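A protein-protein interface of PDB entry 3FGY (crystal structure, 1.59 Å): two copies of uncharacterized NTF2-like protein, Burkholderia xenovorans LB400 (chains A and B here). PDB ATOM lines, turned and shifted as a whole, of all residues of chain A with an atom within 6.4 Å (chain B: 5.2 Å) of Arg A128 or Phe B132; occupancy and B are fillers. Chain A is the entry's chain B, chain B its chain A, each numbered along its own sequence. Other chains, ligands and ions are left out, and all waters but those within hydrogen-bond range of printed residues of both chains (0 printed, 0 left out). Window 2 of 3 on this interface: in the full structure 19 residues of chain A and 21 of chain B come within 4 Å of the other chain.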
ATOM      1  N   GLU A  41       6.085   6.247 -14.109  1.00  0.00           N
ATOM      2  CA  GLU A  41       5.470   5.879 -12.840  1.00  0.00           C
ATOM      3  C   GLU A  41       4.760   4.548 -13.091  1.00  0.00           C
ATOM      4  O   GLU A  41       3.599   4.496 -13.545  1.00  0.00           O
ATOM      5  CB  GLU A  41       4.496   6.963 -12.376  1.00  0.00           C
ATOM      6  CG  GLU A  41       3.839   6.686 -11.011  1.00  0.00           C
ATOM      7  CD  GLU A  41       2.790   7.719 -10.658  1.00  0.00           C
ATOM      8  OE1 GLU A  41       3.154   8.830 -10.234  1.00  0.00           O
ATOM      9  OE2 GLU A  41       1.586   7.404 -10.786  1.00  0.00           O
ATOM     10  N   THR A  95      -3.025  -6.227 -13.007  1.00  0.00           N
ATOM     11  CA  THR A  95      -4.238  -5.551 -13.496  1.00  0.00           C
ATOM     12  C   THR A  95      -4.960  -6.309 -14.623  1.00  0.00           C
ATOM     13  O   THR A  95      -6.144  -6.053 -14.865  1.00  0.00           O
ATOM     14  CB  THR A  95      -3.911  -4.120 -13.980  1.00  0.00           C
ATOM     15  OG1 THR A  95      -2.962  -4.187 -15.045  1.00  0.00           O
ATOM     16  CG2 THR A  95      -3.320  -3.257 -12.859  1.00  0.00           C
ATOM     17  N   ARG A  97      -4.553  -5.729 -17.549  1.00  0.00           N
ATOM     18  CA  ARG A  97      -4.652  -4.704 -18.570  1.00  0.00           C
ATOM     19  C   ARG A  97      -3.507  -4.847 -19.554  1.00  0.00           C
ATOM     20  O   ARG A  97      -2.374  -5.139 -19.197  1.00  0.00           O
ATOM     21  CB  ARG A  97      -4.604  -3.288 -17.983  1.00  0.00           C
ATOM     22  CG  ARG A  97      -5.660  -2.931 -16.951  1.00  0.00           C
ATOM     23  CD  ARG A  97      -5.779  -1.390 -16.793  1.00  0.00           C
ATOM     24  NE  ARG A  97      -6.008  -0.952 -15.406  1.00  0.00           N
ATOM     25  N   THR A 123       5.601   6.390 -21.309  1.00  0.00           N
ATOM     26  CA  THR A 123       5.359   6.362 -19.891  1.00  0.00           C
ATOM     27  C   THR A 123       3.867   6.518 -19.569  1.00  0.00           C
ATOM     28  O   THR A 123       3.403   5.926 -18.616  1.00  0.00           O
ATOM     29  CB  THR A 123       6.222   7.413 -19.148  1.00  0.00           C
ATOM     30  OG1 THR A 123       6.068   8.674 -19.817  1.00  0.00           O
ATOM     31  CG2 THR A 123       7.723   6.977 -19.104  1.00  0.00           C
ATOM     32  N   LEU A 124       3.141   7.320 -20.333  1.00  0.00           N
ATOM     33  CA  LEU A 124       1.697   7.452 -20.130  1.00  0.00           C
ATOM     34  C   LEU A 124       0.976   6.139 -20.315  1.00  0.00           C
ATOM     35  O   LEU A 124       0.180   5.732 -19.486  1.00  0.00           O
ATOM     36  CB  LEU A 124       1.110   8.518 -21.039  1.00  0.00           C
ATOM     37  CG  LEU A 124      -0.391   8.747 -20.919  1.00  0.00           C
ATOM     38  CD1 LEU A 124      -0.774   9.059 -19.473  1.00  0.00           C
ATOM     39  CD2 LEU A 124      -0.786   9.892 -21.875  1.00  0.00           C
ATOM     40  N   ALA A 125       1.285   5.441 -21.401  1.00  0.00           N
ATOM     41  CA  ALA A 125       0.663   4.141 -21.657  1.00  0.00           C
ATOM     42  C   ALA A 125       0.955   3.115 -20.560  1.00  0.00           C
ATOM     43  O   ALA A 125       0.068   2.366 -20.154  1.00  0.00           O
ATOM     44  CB  ALA A 125       1.100   3.596 -22.991  1.00  0.00           C
ATOM     45  N   LEU A 126       2.200   3.077 -20.086  1.00  0.00           N
ATOM     46  CA  LEU A 126       2.582   2.120 -19.037  1.00  0.00           C
ATOM     47  C   LEU A 126       1.918   2.486 -17.703  1.00  0.00           C
ATOM     48  O   LEU A 126       1.501   1.612 -16.957  1.00  0.00           O
ATOM     49  CB  LEU A 126       4.110   1.981 -18.941  1.00  0.00           C
ATOM     50  CG  LEU A 126       4.688   1.156 -20.100  1.00  0.00           C
ATOM     51  CD1 LEU A 126       6.125   1.558 -20.428  1.00  0.00           C
ATOM     52  CD2 LEU A 126       4.589  -0.350 -19.760  1.00  0.00           C
ATOM     53  N   ALA A 127       1.786   3.770 -17.422  1.00  0.00           N
ATOM     54  CA  ALA A 127       1.120   4.224 -16.198  1.00  0.00           C
ATOM     55  C   ALA A 127      -0.339   3.825 -16.205  1.00  0.00           C
ATOM     56  O   ALA A 127      -0.861   3.320 -15.201  1.00  0.00           O
ATOM     57  CB  ALA A 127       1.262   5.727 -16.060  1.00  0.00           C
ATOM     58  N   ARG A 128      -0.994   4.031 -17.338  1.00  0.00           N
ATOM     59  CA  ARG A 128      -2.415   3.653 -17.463  1.00  0.00           C
ATOM     60  C   ARG A 128      -2.615   2.165 -17.238  1.00  0.00           C
ATOM     61  O   ARG A 128      -3.611   1.754 -16.625  1.00  0.00           O
ATOM     62  CB  ARG A 128      -2.974   4.044 -18.820  1.00  0.00           C
ATOM     63  CG  ARG A 128      -3.116   5.528 -19.015  1.00  0.00           C
ATOM     64  CD  ARG A 128      -4.387   5.892 -19.712  1.00  0.00           C
ATOM     65  NE  ARG A 128      -4.668   7.309 -19.513  1.00  0.00           N
ATOM     66  CZ  ARG A 128      -4.507   8.246 -20.431  1.00  0.00           C
ATOM     67  NH1 ARG A 128      -4.087   7.918 -21.629  1.00  0.00           N
ATOM     68  NH2 ARG A 128      -4.785   9.514 -20.140  1.00  0.00           N
ATOM     69  N   ALA A 129      -1.707   1.352 -17.747  1.00  0.00           N
ATOM     70  CA  ALA A 129      -1.842  -0.106 -17.685  1.00  0.00           C
ATOM     71  C   ALA A 129      -1.626  -0.617 -16.277  1.00  0.00           C
ATOM     72  O   ALA A 129      -2.030  -1.734 -15.935  1.00  0.00           O
ATOM     73  CB  ALA A 129      -0.832  -0.772 -18.599  1.00  0.00           C
ATOM     74  N   THR A 130      -0.928   0.163 -15.461  1.00  0.00           N
ATOM     75  CA  THR A 130      -0.579  -0.299 -14.132  1.00  0.00           C
ATOM     76  C   THR A 130      -1.369   0.457 -13.057  1.00  0.00           C
ATOM     77  O   THR A 130      -1.325   0.087 -11.887  1.00  0.00           O
ATOM     78  CB  THR A 130       0.975  -0.272 -13.928  1.00  0.00           C
ATOM     79  OG1 THR A 130       1.490   1.030 -14.172  1.00  0.00           O
ATOM     80  CG2 THR A 130       1.661  -1.232 -14.899  1.00  0.00           C
ATOM     81  N   ASN A 131      -2.128   1.470 -13.473  1.00  0.00           N
ATOM     82  CA  ASN A 131      -2.889   2.352 -12.576  1.00  0.00           C
ATOM     83  C   ASN A 131      -1.983   3.084 -11.602  1.00  0.00           C
ATOM     84  O   ASN A 131      -1.141   3.881 -12.026  1.00  0.00           O
ATOM     85  CB  ASN A 131      -3.989   1.576 -11.845  1.00  0.00           C
ATOM     86  CG  ASN A 131      -4.863   0.777 -12.792  1.00  0.00           C
ATOM     87  OD1 ASN A 131      -5.150   1.213 -13.906  1.00  0.00           O
ATOM     88  ND2 ASN A 131      -5.296  -0.404 -12.351  1.00  0.00           N
ATOM     89  N   GLU B  41      -0.564  11.996 -25.087  1.00  0.00           N
ATOM     90  CA  GLU B  41      -1.842  12.739 -25.060  1.00  0.00           C
ATOM     91  C   GLU B  41      -1.557  14.125 -24.540  1.00  0.00           C
ATOM     92  O   GLU B  41      -1.456  14.363 -23.318  1.00  0.00           O
ATOM     93  CB  GLU B  41      -2.851  12.023 -24.178  1.00  0.00           C
ATOM     94  CG  GLU B  41      -3.116  10.596 -24.620  1.00  0.00           C
ATOM     95  CD  GLU B  41      -4.124   9.897 -23.760  1.00  0.00           C
ATOM     96  OE1 GLU B  41      -4.697  10.520 -22.828  1.00  0.00           O
ATOM     97  OE2 GLU B  41      -4.334   8.699 -24.036  1.00  0.00           O
ATOM     98  N   TRP B  42      -1.320  15.024 -25.492  1.00  0.00           N
ATOM     99  CA  TRP B  42      -0.935  16.386 -25.216  1.00  0.00           C
ATOM    100  C   TRP B  42      -1.103  17.115 -26.550  1.00  0.00           C
ATOM    101  O   TRP B  42      -1.329  16.466 -27.577  1.00  0.00           O
ATOM    102  CB  TRP B  42       0.480  16.484 -24.663  1.00  0.00           C
ATOM    103  CG  TRP B  42       1.617  16.032 -25.540  1.00  0.00           C
ATOM    104  CD1 TRP B  42       1.832  14.776 -26.073  1.00  0.00           C
ATOM    105  CD2 TRP B  42       2.757  16.812 -25.902  1.00  0.00           C
ATOM    106  NE1 TRP B  42       3.022  14.752 -26.748  1.00  0.00           N
ATOM    107  CE2 TRP B  42       3.594  15.995 -26.697  1.00  0.00           C
ATOM    108  CE3 TRP B  42       3.134  18.138 -25.677  1.00  0.00           C
ATOM    109  CZ2 TRP B  42       4.797  16.450 -27.210  1.00  0.00           C
ATOM    110  CZ3 TRP B  42       4.325  18.586 -26.212  1.00  0.00           C
ATOM    111  CH2 TRP B  42       5.158  17.735 -26.939  1.00  0.00           C
ATOM    112  N   LEU B 124       3.936  10.600 -20.029  1.00  0.00           N
ATOM    113  CA  LEU B 124       3.241  10.858 -18.754  1.00  0.00           C
ATOM    114  C   LEU B 124       3.513  12.275 -18.261  1.00  0.00           C
ATOM    115  O   LEU B 124       2.616  12.995 -17.888  1.00  0.00           O
ATOM    116  CB  LEU B 124       3.685   9.834 -17.709  1.00  0.00           C
ATOM    117  CG  LEU B 124       3.046   9.998 -16.328  1.00  0.00           C
ATOM    118  CD1 LEU B 124       1.498  10.007 -16.394  1.00  0.00           C
ATOM    119  CD2 LEU B 124       3.540   8.958 -15.362  1.00  0.00           C
ATOM    120  N   ALA B 127       1.721  14.835 -20.564  1.00  0.00           N
ATOM    121  CA  ALA B 127       0.268  14.800 -20.326  1.00  0.00           C
ATOM    122  C   ALA B 127      -0.055  15.571 -19.042  1.00  0.00           C
ATOM    123  O   ALA B 127      -0.956  16.415 -19.024  1.00  0.00           O
ATOM    124  CB  ALA B 127      -0.264  13.358 -20.257  1.00  0.00           C
ATOM    125  N   ARG B 128       0.675  15.298 -17.963  1.00  0.00           N
ATOM    126  CA  ARG B 128       0.448  15.983 -16.705  1.00  0.00           C
ATOM    127  C   ARG B 128       0.624  17.484 -16.863  1.00  0.00           C
ATOM    128  O   ARG B 128      -0.194  18.266 -16.401  1.00  0.00           O
ATOM    129  CB  ARG B 128       1.370  15.433 -15.638  1.00  0.00           C
ATOM    130  CG  ARG B 128       0.950  14.105 -15.149  1.00  0.00           C
ATOM    131  CD  ARG B 128       1.986  13.499 -14.282  1.00  0.00           C
ATOM    132  NE  ARG B 128       1.465  12.381 -13.506  1.00  0.00           N
ATOM    133  CZ  ARG B 128       2.234  11.564 -12.779  1.00  0.00           C
ATOM    134  NH1 ARG B 128       3.568  11.691 -12.741  1.00  0.00           N
ATOM    135  NH2 ARG B 128       1.665  10.609 -12.088  1.00  0.00           N
ATOM    136  N   THR B 130       0.443  19.398 -19.413  1.00  0.00           N
ATOM    137  CA  THR B 130      -0.520  20.044 -20.320  1.00  0.00           C
ATOM    138  C   THR B 130      -1.956  19.796 -19.883  1.00  0.00           C
ATOM    139  O   THR B 130      -2.899  20.202 -20.585  1.00  0.00           O
ATOM    140  CB  THR B 130      -0.314  19.561 -21.778  1.00  0.00           C
ATOM    141  OG1 THR B 130      -0.561  18.142 -21.865  1.00  0.00           O
ATOM    142  CG2 THR B 130       1.111  19.867 -22.242  1.00  0.00           C
ATOM    143  N   ASN B 131      -2.139  19.132 -18.742  1.00  0.00           N
ATOM    144  CA  ASN B 131      -3.457  18.801 -18.223  1.00  0.00           C
ATOM    145  C   ASN B 131      -4.224  17.880 -19.191  1.00  0.00           C
ATOM    146  O   ASN B 131      -5.461  17.924 -19.259  1.00  0.00           O
ATOM    147  CB  ASN B 131      -4.229  20.094 -17.885  1.00  0.00           C
ATOM    148  CG  ASN B 131      -5.354  19.865 -16.915  1.00  0.00           C
ATOM    149  OD1 ASN B 131      -5.224  19.086 -15.980  1.00  0.00           O
ATOM    150  ND2 ASN B 131      -6.481  20.545 -17.134  1.00  0.00           N
ATOM    151  N   PHE B 132      -3.462  17.061 -19.924  1.00  0.00           N
ATOM    152  CA  PHE B 132      -3.934  15.984 -20.826  1.00  0.00           C
ATOM    153  C   PHE B 132      -4.625  16.502 -22.091  1.00  0.00           C
ATOM    154  O   PHE B 132      -5.491  15.822 -22.680  1.00  0.00           O
ATOM    155  CB  PHE B 132      -4.796  14.954 -20.063  1.00  0.00           C
ATOM    156  CG  PHE B 132      -4.026  14.185 -19.001  1.00  0.00           C
ATOM    157  CD1 PHE B 132      -3.682  14.786 -17.801  1.00  0.00           C
ATOM    158  CD2 PHE B 132      -3.665  12.853 -19.208  1.00  0.00           C
ATOM    159  CE1 PHE B 132      -2.973  14.086 -16.818  1.00  0.00           C
ATOM    160  CE2 PHE B 132      -2.966  12.143 -18.238  1.00  0.00           C
ATOM    161  CZ  PHE B 132      -2.611  12.767 -17.038  1.00  0.00           C
ATOM    162  N   ASN B 133      -4.194  17.677 -22.535  1.00  0.00           N
ATOM    163  CA  ASN B 133      -4.855  18.399 -23.609  1.00  0.00           C
ATOM    164  C   ASN B 133      -4.466  17.765 -24.924  1.00  0.00           C
ATOM    165  O   ASN B 133      -3.474  18.133 -25.518  1.00  0.00           O
ATOM    166  CB  ASN B 133      -4.449  19.885 -23.578  1.00  0.00           C
ATOM    167  CG  ASN B 133      -5.289  20.766 -24.511  1.00  0.00           C
ATOM    168  OD1 ASN B 133      -6.203  20.291 -25.205  1.00  0.00           O
ATOM    169  ND2 ASN B 133      -4.977  22.067 -24.522  1.00  0.00           N
ATOM    170  N   ALA B 134      -5.254  16.799 -25.370  1.00  0.00           N
ATOM    171  CA  ALA B 134      -5.029  16.174 -26.665  1.00  0.00           C
ATOM    172  C   ALA B 134      -5.252  17.133 -27.862  1.00  0.00           C
ATOM    173  O   ALA B 134      -4.950  16.767 -29.002  1.00  0.00           O
ATOM    174  CB  ALA B 134      -5.907  14.923 -26.797  1.00  0.00           C
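Glu A41 touches Leu B124, and with the chains exchanged Leu A124 touches Glu B41.
Glu A41 touches Arg B128, and with the chains exchanged Arg A128 touches Glu B41.
Leu A124 touches its own counterpart, Leu B124.
Leu A124 touches Ala B127, but with the chains exchanged Ala A127 does not touch Leu B124 (4.01 Å).
Of the 9 pairs that touch across the chains among the printed residues, 5 have their exchanged pair printed and touching as well.
CD2 of Leu B124 touches CB of Glu A41 (3.7 Å).
Glu B41 touches Leu A124 (CG to CD2, 3.7 Å).
CD2 of Leu A124 touches CB of Ala B127, at 3.9 Å.
Phe B132 touches Leu A124 (CE2 to CD1, 3.98 Å).
NH2 of Arg A128 touches CD2 of Phe B132 (3.6 Å).
The side-chain carboxylate (OE2) of Glu B41 lies within salt-bridge range of the guanidinium group (NH1) of Arg A128 (2.5 Å).
The backbone NH of Leu B124 is in hydrogen-bond range of the side-chain hydroxyl of Thr A123, at 2.9 Å.
The guanidinium group (NH2) of Arg B128 is in salt-bridge range of the side-chain carboxylate (OE1) of Glu A41 (3.0 Å).
The backbone NH (N) of Leu B124 lies close to the backbone NH (N) of Leu A124 (3.4 Å).
Of the 12 printed residues of chain A, 4 touch a printed residue of chain B.
Hydrophobic or aromatic side chains of chain A that line the printed part of chain B: Leu A124.
Hydrophobic or aromatic side chains of chain B that line the printed part of chain A: Leu B124, Ala B127 and Phe B132.
Among the printed residues, Asp or Glu carboxylates within 4 Å of a Lys or Arg side-chain nitrogen of the other chain: Glu A41 with Arg B128 and Arg A128 with Glu B41.
Of the printed residues of chain B, Thr A123 touches Leu B124.
Of the printed residues of chain B, Leu A124 touches Glu B41 (3.7 Å), Leu B124 (3.4 Å), Ala B127 (3.9 Å) and Phe B132 (3.98 Å).
Leu A126 touches none of the printed residues of chain B.
Of chain B, only Glu B41 and Phe B132 come within 4 Å of Arg A128.
Of the printed residues of chain A, Ala B127 touches Leu A124 (3.9 Å).
Of the printed residues of chain A, Phe B132 touches Leu A124 and Arg A128.
The nearest printed residue of chain B that does not touch Arg A128 is Ala B127 (5.9 Å).
The nearest printed residue of chain A that does not touch Phe B132 is Ala A127 (8.0 Å).
The nearest printed residue of chain A that does not touch Leu B124 is Ala A127 (4.01 Å).
The side-chain hydroxyl (OG1) of Thr B130 is in hydrogen-bond range of the backbone carbonyl oxygen (O) of Ala B127 (3.3 Å).
The backbone NH (N) of Phe B132 sits at hydrogen-bond distance from the backbone carbonyl oxygen (O) of Ala B127, at 2.7 Å.
O of Arg A128 lies close to OD1 of Asn A131.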
